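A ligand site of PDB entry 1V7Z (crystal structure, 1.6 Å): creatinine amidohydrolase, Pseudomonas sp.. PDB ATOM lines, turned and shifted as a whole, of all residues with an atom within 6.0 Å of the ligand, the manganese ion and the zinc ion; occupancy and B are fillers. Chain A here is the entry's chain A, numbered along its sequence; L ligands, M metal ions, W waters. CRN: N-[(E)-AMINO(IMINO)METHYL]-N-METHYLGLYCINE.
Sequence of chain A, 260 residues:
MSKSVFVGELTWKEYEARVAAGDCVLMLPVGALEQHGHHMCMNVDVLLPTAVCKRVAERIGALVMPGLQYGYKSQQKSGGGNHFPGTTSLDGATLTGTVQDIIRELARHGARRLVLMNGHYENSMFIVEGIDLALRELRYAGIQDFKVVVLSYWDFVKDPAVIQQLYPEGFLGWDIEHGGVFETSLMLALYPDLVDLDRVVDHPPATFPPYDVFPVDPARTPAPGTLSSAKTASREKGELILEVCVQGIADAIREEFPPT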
ATOM      1  N   ALA A  32      27.372  -5.513   7.244  1.00  0.00           N
ATOM      2  CA  ALA A  32      25.943  -5.766   7.082  1.00  0.00           C
ATOM      3  C   ALA A  32      25.522  -5.353   5.688  1.00  0.00           C
ATOM      4  O   ALA A  32      26.220  -4.587   5.025  1.00  0.00           O
ATOM      5  CB  ALA A  32      25.135  -4.979   8.106  1.00  0.00           C
ATOM      6  N   GLU A  34      22.283  -3.463   4.553  1.00  0.00           N
ATOM      7  CA  GLU A  34      21.295  -2.718   5.316  1.00  0.00           C
ATOM      8  C   GLU A  34      20.942  -1.430   4.595  1.00  0.00           C
ATOM      9  O   GLU A  34      21.815  -0.738   4.076  1.00  0.00           O
ATOM     10  CB  GLU A  34      21.866  -2.375   6.683  1.00  0.00           C
ATOM     11  CG  GLU A  34      20.905  -1.677   7.628  1.00  0.00           C
ATOM     12  CD  GLU A  34      21.575  -1.224   8.911  1.00  0.00           C
ATOM     13  OE1 GLU A  34      20.932  -1.241   9.973  1.00  0.00           O
ATOM     14  OE2 GLU A  34      22.769  -0.853   8.862  1.00  0.00           O
ATOM     15  N   HIS A  36      20.321   2.295   3.838  1.00  0.00           N
ATOM     16  CA  HIS A  36      20.985   3.511   4.297  1.00  0.00           C
ATOM     17  C   HIS A  36      20.380   4.751   3.621  1.00  0.00           C
ATOM     18  O   HIS A  36      21.089   5.588   3.087  1.00  0.00           O
ATOM     19  CB  HIS A  36      22.479   3.424   4.015  1.00  0.00           C
ATOM     20  CG  HIS A  36      23.248   2.665   5.061  1.00  0.00           C
ATOM     21  ND1 HIS A  36      23.408   1.297   5.025  1.00  0.00           N
ATOM     22  CD2 HIS A  36      23.900   3.093   6.159  1.00  0.00           C
ATOM     23  CE1 HIS A  36      24.135   0.909   6.059  1.00  0.00           C
ATOM     24  NE2 HIS A  36      24.451   1.989   6.767  1.00  0.00           N
ATOM     25  N   VAL A  44      27.321  -0.210   2.696  1.00  0.00           N
ATOM     26  CA  VAL A  44      28.144   0.756   3.441  1.00  0.00           C
ATOM     27  C   VAL A  44      28.895   0.133   4.613  1.00  0.00           C
ATOM     28  O   VAL A  44      30.082   0.379   4.798  1.00  0.00           O
ATOM     29  CB  VAL A  44      27.289   1.943   3.980  1.00  0.00           C
ATOM     30  CG1 VAL A  44      28.072   2.789   4.985  1.00  0.00           C
ATOM     31  CG2 VAL A  44      26.808   2.828   2.838  1.00  0.00           C
ATOM     32  N   ASP A  45      28.212  -0.693   5.402  1.00  0.00           N
ATOM     33  CA  ASP A  45      28.787  -1.238   6.626  1.00  0.00           C
ATOM     34  C   ASP A  45      29.896  -2.274   6.393  1.00  0.00           C
ATOM     35  O   ASP A  45      30.631  -2.616   7.323  1.00  0.00           O
ATOM     36  CB  ASP A  45      27.695  -1.868   7.497  1.00  0.00           C
ATOM     37  CG  ASP A  45      26.757  -0.839   8.104  1.00  0.00           C
ATOM     38  OD1 ASP A  45      26.897   0.392   7.821  1.00  0.00           O
ATOM     39  OD2 ASP A  45      25.840  -1.175   8.887  1.00  0.00           O
ATOM     40  N   SER A  78      18.894   2.242  16.258  1.00  0.00           N
ATOM     41  CA  SER A  78      20.254   2.368  15.740  1.00  0.00           C
ATOM     42  C   SER A  78      20.399   2.219  14.218  1.00  0.00           C
ATOM     43  O   SER A  78      21.395   2.640  13.663  1.00  0.00           O
ATOM     44  CB  SER A  78      21.201   1.380  16.447  1.00  0.00           C
ATOM     45  OG  SER A  78      20.658   0.067  16.480  1.00  0.00           O
ATOM     46  N   GLY A  79      19.442   1.593  13.552  1.00  0.00           N
ATOM     47  CA  GLY A  79      19.557   1.298  12.131  1.00  0.00           C
ATOM     48  C   GLY A  79      18.261   1.388  11.345  1.00  0.00           C
ATOM     49  O   GLY A  79      18.220   0.971  10.192  1.00  0.00           O
ATOM     50  N   GLY A 119      31.571  -2.650  11.624  1.00  0.00           N
ATOM     51  CA  GLY A 119      31.015  -1.517  10.907  1.00  0.00           C
ATOM     52  C   GLY A 119      29.507  -1.374  10.989  1.00  0.00           C
ATOM     53  O   GLY A 119      28.952  -0.453  10.409  1.00  0.00           O
ATOM     54  N   HIS A 120      28.841  -2.265  11.740  1.00  0.00           N
ATOM     55  CA  HIS A 120      27.392  -2.245  11.894  1.00  0.00           C
ATOM     56  C   HIS A 120      27.085  -2.339  13.380  1.00  0.00           C
ATOM     57  O   HIS A 120      27.433  -3.313  14.055  1.00  0.00           O
ATOM     58  CB  HIS A 120      26.806  -3.418  11.126  1.00  0.00           C
ATOM     59  CG  HIS A 120      25.334  -3.647  11.323  1.00  0.00           C
ATOM     60  ND1 HIS A 120      24.357  -2.854  10.760  1.00  0.00           N
ATOM     61  CD2 HIS A 120      24.691  -4.661  11.951  1.00  0.00           C
ATOM     62  CE1 HIS A 120      23.169  -3.366  11.054  1.00  0.00           C
ATOM     63  NE2 HIS A 120      23.343  -4.471  11.753  1.00  0.00           N
ATOM     64  N   TYR A 121      26.465  -1.281  13.900  1.00  0.00           N
ATOM     65  CA  TYR A 121      26.274  -1.068  15.321  1.00  0.00           C
ATOM     66  C   TYR A 121      25.748  -2.303  16.056  1.00  0.00           C
ATOM     67  O   TYR A 121      26.253  -2.688  17.109  1.00  0.00           O
ATOM     68  CB  TYR A 121      25.301   0.094  15.511  1.00  0.00           C
ATOM     69  CG  TYR A 121      25.249   0.646  16.898  1.00  0.00           C
ATOM     70  CD1 TYR A 121      26.045   1.734  17.257  1.00  0.00           C
ATOM     71  CD2 TYR A 121      24.395   0.113  17.854  1.00  0.00           C
ATOM     72  CE1 TYR A 121      26.000   2.266  18.527  1.00  0.00           C
ATOM     73  CE2 TYR A 121      24.339   0.639  19.132  1.00  0.00           C
ATOM     74  CZ  TYR A 121      25.149   1.713  19.469  1.00  0.00           C
ATOM     75  OH  TYR A 121      25.096   2.243  20.728  1.00  0.00           O
ATOM     76  N   GLU A 122      24.762  -2.947  15.442  1.00  0.00           N
ATOM     77  CA  GLU A 122      24.048  -4.052  16.071  1.00  0.00           C
ATOM     78  C   GLU A 122      24.853  -5.347  16.206  1.00  0.00           C
ATOM     79  O   GLU A 122      24.444  -6.256  16.921  1.00  0.00           O
ATOM     80  CB  GLU A 122      22.779  -4.347  15.249  1.00  0.00           C
ATOM     81  CG  GLU A 122      21.675  -3.307  15.339  1.00  0.00           C
ATOM     82  CD  GLU A 122      21.794  -2.146  14.356  1.00  0.00           C
ATOM     83  OE1 GLU A 122      22.859  -1.922  13.757  1.00  0.00           O
ATOM     84  OE2 GLU A 122      20.782  -1.428  14.197  1.00  0.00           O
ATOM     85  N   TYR A 153      34.726   1.144  14.408  1.00  0.00           N
ATOM     86  CA  TYR A 153      35.736   2.121  13.948  1.00  0.00           C
ATOM     87  C   TYR A 153      35.402   3.564  14.316  1.00  0.00           C
ATOM     88  O   TYR A 153      36.307   4.368  14.591  1.00  0.00           O
ATOM     89  CB  TYR A 153      36.054   1.953  12.446  1.00  0.00           C
ATOM     90  CG  TYR A 153      34.920   2.356  11.542  1.00  0.00           C
ATOM     91  CD1 TYR A 153      34.852   3.641  11.021  1.00  0.00           C
ATOM     92  CD2 TYR A 153      33.910   1.462  11.220  1.00  0.00           C
ATOM     93  CE1 TYR A 153      33.813   4.024  10.215  1.00  0.00           C
ATOM     94  CE2 TYR A 153      32.860   1.839  10.421  1.00  0.00           C
ATOM     95  CZ  TYR A 153      32.804   3.118   9.911  1.00  0.00           C
ATOM     96  OH  TYR A 153      31.754   3.495   9.112  1.00  0.00           O
ATOM     97  N   TRP A 154      34.111   3.906  14.354  1.00  0.00           N
ATOM     98  CA  TRP A 154      33.677   5.254  14.746  1.00  0.00           C
ATOM     99  C   TRP A 154      34.045   5.660  16.168  1.00  0.00           C
ATOM    100  O   TRP A 154      34.158   6.849  16.452  1.00  0.00           O
ATOM    101  CB  TRP A 154      32.164   5.432  14.545  1.00  0.00           C
ATOM    102  CG  TRP A 154      31.315   4.360  15.194  1.00  0.00           C
ATOM    103  CD1 TRP A 154      30.950   4.277  16.505  1.00  0.00           C
ATOM    104  CD2 TRP A 154      30.723   3.230  14.537  1.00  0.00           C
ATOM    105  NE1 TRP A 154      30.179   3.161  16.706  1.00  0.00           N
ATOM    106  CE2 TRP A 154      30.021   2.501  15.517  1.00  0.00           C
ATOM    107  CE3 TRP A 154      30.730   2.762  13.219  1.00  0.00           C
ATOM    108  CZ2 TRP A 154      29.323   1.331  15.225  1.00  0.00           C
ATOM    109  CZ3 TRP A 154      30.032   1.592  12.927  1.00  0.00           C
ATOM    110  CH2 TRP A 154      29.341   0.900  13.927  1.00  0.00           C
ATOM    111  N   TRP A 174      26.473   7.789  18.660  1.00  0.00           N
ATOM    112  CA  TRP A 174      26.749   6.923  17.518  1.00  0.00           C
ATOM    113  C   TRP A 174      25.548   6.042  17.129  1.00  0.00           C
ATOM    114  O   TRP A 174      25.466   5.603  15.996  1.00  0.00           O
ATOM    115  CB  TRP A 174      27.991   6.062  17.778  1.00  0.00           C
ATOM    116  CG  TRP A 174      29.268   6.862  17.867  1.00  0.00           C
ATOM    117  CD1 TRP A 174      30.138   6.898  18.914  1.00  0.00           C
ATOM    118  CD2 TRP A 174      29.806   7.736  16.871  1.00  0.00           C
ATOM    119  NE1 TRP A 174      31.195   7.736  18.635  1.00  0.00           N
ATOM    120  CE2 TRP A 174      31.020   8.266  17.383  1.00  0.00           C
ATOM    121  CE3 TRP A 174      29.395   8.132  15.589  1.00  0.00           C
ATOM    122  CZ2 TRP A 174      31.808   9.170  16.660  1.00  0.00           C
ATOM    123  CZ3 TRP A 174      30.190   9.017  14.874  1.00  0.00           C
ATOM    124  CH2 TRP A 174      31.378   9.531  15.420  1.00  0.00           C
ATOM    125  N   ASP A 175      24.628   5.813  18.066  1.00  0.00           N
ATOM    126  CA  ASP A 175      23.380   5.079  17.768  1.00  0.00           C
ATOM    127  C   ASP A 175      22.504   5.693  16.653  1.00  0.00           C
ATOM    128  O   ASP A 175      22.083   4.992  15.736  1.00  0.00           O
ATOM    129  CB  ASP A 175      22.533   4.856  19.041  1.00  0.00           C
ATOM    130  CG  ASP A 175      22.304   6.133  19.834  1.00  0.00           C
ATOM    131  OD1 ASP A 175      21.129   6.533  19.968  1.00  0.00           O
ATOM    132  OD2 ASP A 175      23.231   6.792  20.346  1.00  0.00           O
ATOM    133  N   ILE A 176      22.219   6.999  16.705  1.00  0.00           N
ATOM    134  CA  ILE A 176      21.410   7.607  15.644  1.00  0.00           C
ATOM    135  C   ILE A 176      22.232   8.047  14.426  1.00  0.00           C
ATOM    136  O   ILE A 176      21.702   8.677  13.507  1.00  0.00           O
ATOM    137  CB  ILE A 176      20.516   8.752  16.188  1.00  0.00           C
ATOM    138  CG1 ILE A 176      21.365   9.878  16.781  1.00  0.00           C
ATOM    139  CG2 ILE A 176      19.544   8.211  17.213  1.00  0.00           C
ATOM    140  CD1 ILE A 176      20.687  11.233  16.661  1.00  0.00           C
ATOM    141  N   GLU A 177      23.509   7.675  14.411  1.00  0.00           N
ATOM    142  CA  GLU A 177      24.395   7.959  13.301  1.00  0.00           C
ATOM    143  C   GLU A 177      24.247   6.893  12.215  1.00  0.00           C
ATOM    144  O   GLU A 177      25.217   6.240  11.808  1.00  0.00           O
ATOM    145  CB  GLU A 177      25.846   8.038  13.787  1.00  0.00           C
ATOM    146  CG  GLU A 177      26.770   8.791  12.866  1.00  0.00           C
ATOM    147  CD  GLU A 177      26.130  10.029  12.275  1.00  0.00           C
ATOM    148  OE1 GLU A 177      25.834  10.976  13.035  1.00  0.00           O
ATOM    149  OE2 GLU A 177      25.886  10.043  11.060  1.00  0.00           O
ATOM    150  N   HIS A 178      23.032   6.716  11.736  1.00  0.00           N
ATOM    151  CA  HIS A 178      22.760   5.755  10.676  1.00  0.00           C
ATOM    152  C   HIS A 178      22.399   6.488   9.394  1.00  0.00           C
ATOM    153  O   HIS A 178      21.317   7.055   9.287  1.00  0.00           O
ATOM    154  CB  HIS A 178      21.639   4.808  11.078  1.00  0.00           C
ATOM    155  CG  HIS A 178      21.341   3.801  10.025  1.00  0.00           C
ATOM    156  ND1 HIS A 178      22.280   2.891   9.585  1.00  0.00           N
ATOM    157  CD2 HIS A 178      20.242   3.594   9.263  1.00  0.00           C
ATOM    158  CE1 HIS A 178      21.773   2.165   8.615  1.00  0.00           C
ATOM    159  NE2 HIS A 178      20.533   2.576   8.396  1.00  0.00           N
ATOM    160  N   GLY A 179      23.309   6.458   8.428  1.00  0.00           N
ATOM    161  CA  GLY A 179      23.107   7.111   7.153  1.00  0.00           C
ATOM    162  C   GLY A 179      23.194   8.629   7.234  1.00  0.00           C
ATOM    163  O   GLY A 179      22.731   9.321   6.339  1.00  0.00           O
ATOM    164  N   PHE A 182      28.262  11.162   9.310  1.00  0.00           N
ATOM    165  CA  PHE A 182      29.485  10.379   9.467  1.00  0.00           C
ATOM    166  C   PHE A 182      29.701   9.408   8.304  1.00  0.00           C
ATOM    167  O   PHE A 182      30.713   9.459   7.611  1.00  0.00           O
ATOM    168  CB  PHE A 182      29.431   9.609  10.795  1.00  0.00           C
ATOM    169  CG  PHE A 182      30.666   8.799  11.073  1.00  0.00           C
ATOM    170  CD1 PHE A 182      30.719   7.463  10.722  1.00  0.00           C
ATOM    171  CD2 PHE A 182      31.772   9.367  11.707  1.00  0.00           C
ATOM    172  CE1 PHE A 182      31.846   6.704  10.979  1.00  0.00           C
ATOM    173  CE2 PHE A 182      32.904   8.598  11.962  1.00  0.00           C
ATOM    174  CZ  PHE A 182      32.937   7.265  11.597  1.00  0.00           C
ATOM    175  N   GLU A 183      28.735   8.524   8.095  1.00  0.00           N
ATOM    176  CA  GLU A 183      28.880   7.507   7.055  1.00  0.00           C
ATOM    177  C   GLU A 183      28.857   8.133   5.675  1.00  0.00           C
ATOM    178  O   GLU A 183      29.623   7.736   4.809  1.00  0.00           O
ATOM    179  CB  GLU A 183      27.768   6.458   7.149  1.00  0.00           C
ATOM    180  CG  GLU A 183      27.943   5.522   8.336  1.00  0.00           C
ATOM    181  CD  GLU A 183      26.889   4.429   8.372  1.00  0.00           C
ATOM    182  OE1 GLU A 183      27.290   3.264   8.483  1.00  0.00           O
ATOM    183  OE2 GLU A 183      25.689   4.734   8.307  1.00  0.00           O
ATOM    184  N   LEU A 227      18.462   7.895  10.478  1.00  0.00           N
ATOM    185  CA  LEU A 227      18.140   8.364  11.827  1.00  0.00           C
ATOM    186  C   LEU A 227      18.613   9.800  12.042  1.00  0.00           C
ATOM    187  O   LEU A 227      18.262  10.433  13.022  1.00  0.00           O
ATOM    188  CB  LEU A 227      18.741   7.423  12.879  1.00  0.00           C
ATOM    189  CG  LEU A 227      18.124   6.007  12.899  1.00  0.00           C
ATOM    190  CD1 LEU A 227      18.727   5.173  14.013  1.00  0.00           C
ATOM    191  CD2 LEU A 227      16.602   6.050  13.033  1.00  0.00           C
HETATM  192  O9  CRN L   1      25.726   0.506  11.756  1.00  0.00           O
HETATM  193  C7  CRN L   1      25.635   1.519  11.035  1.00  0.00           C
HETATM  194  O8  CRN L   1      24.957   1.521   9.970  1.00  0.00           O
HETATM  195  C5  CRN L   1      26.320   2.803  11.470  1.00  0.00           C
HETATM  196  N1  CRN L   1      25.942   3.244  12.824  1.00  0.00           N
HETATM  197  C4  CRN L   1      27.024   3.842  13.613  1.00  0.00           C
HETATM  198  C2  CRN L   1      24.698   3.134  13.305  1.00  0.00           C
HETATM  199  N6  CRN L   1      24.416   3.562  14.458  1.00  0.00           N
HETATM  200  N3  CRN L   1      23.716   2.580  12.574  1.00  0.00           N
HETATM  201 MN    MN M   1      24.346  -0.657  10.202  1.00  0.00          MN
HETATM  202 ZN    ZN M   2      25.788   1.966   8.268  1.00  0.00          ZN
HETATM  203  O   HOH W   1      22.773  -0.167  11.766  1.00  0.00           O
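ND1 of His 178 sits at hydrogen-bond distance from N3 of the ligand (3.3 Å). N6 of the ligand sits at hydrogen-bond distance from O of Trp 174. The backbone carbonyl oxygen of Ser 78 is in hydrogen-bond range of a nitrogen (N3) of the ligand, at 2.6 Å. N of Tyr 121 lies close to O9 of the ligand, 2.9 Å away. The backbone carbonyl oxygen of Asp 175 sits at hydrogen-bond distance from a nitrogen (N6) of the ligand (3.0 Å).
N of Leu 227 is in hydrogen-bond range of O of His 178 (3.2 Å). O of Glu 34 lies within hydrogen-bond range of ND1 of His 36 (2.8 Å). A ring nitrogen (NE2) of His 178 lies within hydrogen-bond range of the backbone carbonyl oxygen (O) of Gly 79, at 3.3 Å. OE2 of Glu 177 sits at hydrogen-bond distance from N of Phe 182 (3.2 Å). N of Gly 179 lies within hydrogen-bond range of OE2 of Glu 183. NE2 of His 120 lies close to OE1 of Glu 122 (3.3 Å). The side-chain hydroxyl (OG) of Ser 78 sits at hydrogen-bond distance from the side-chain carboxylate (OE2) of Glu 122 (2.7 Å).
O of Glu 177 lies close to N1 of the ligand, 3.2 Å away. Residues that only touch the ligand: Gly 119 and Trp 154. Hydrophobic or aromatic side chains within 4 Å of the ligand: Tyr 121, Trp 154 and His 178. 13 residues have an atom within 4 Å of the ligand: Glu 34, His 36, Asp 45, Ser 78, Gly 119, His 120, Tyr 121, Trp 154, Trp 174, Asp 175, Glu 177, His 178 and Glu 183.
The nearest printed residue that does not touch the manganese ion is Glu 122 (4.1 Å).
Residues that only touch the zinc ion: His 178 (3.9 Å).
OD2 of Asp 45 binds the manganese ion, 2.1 Å away. The manganese ion is bound by OE2 of Glu 34. A ring nitrogen (ND1) of His 120 binds the manganese ion, at 2.3 Å. Water W1 is bound to the manganese ion (2.3 Å). O8 of the ligand is bound to the manganese ion. An oxygen (O9) of the ligand is bound to the manganese ion (2.4 Å). The manganese ion has six donor atoms within binding distance.
The zinc ion is bound by O8 of the ligand (1.9 Å), OD1 of Asp 45 (2.0 Å), OE1 of Glu 183 (2.0 Å) and NE2 of His 36 (2.0 Å). The zinc ion has four donor atoms within binding distance. Slightly farther from the zinc ion lies the side-chain carboxylate (OE2) of Glu 183 (2.8 Å).
Water W1 lies within hydrogen-bond range of the side-chain carboxylate (OE1) of Glu 122 (2.7 Å), the side-chain carboxylate (OE1) of Glu 34 (2.8 Å) and a nitrogen (N3) of the ligand (3.0 Å).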
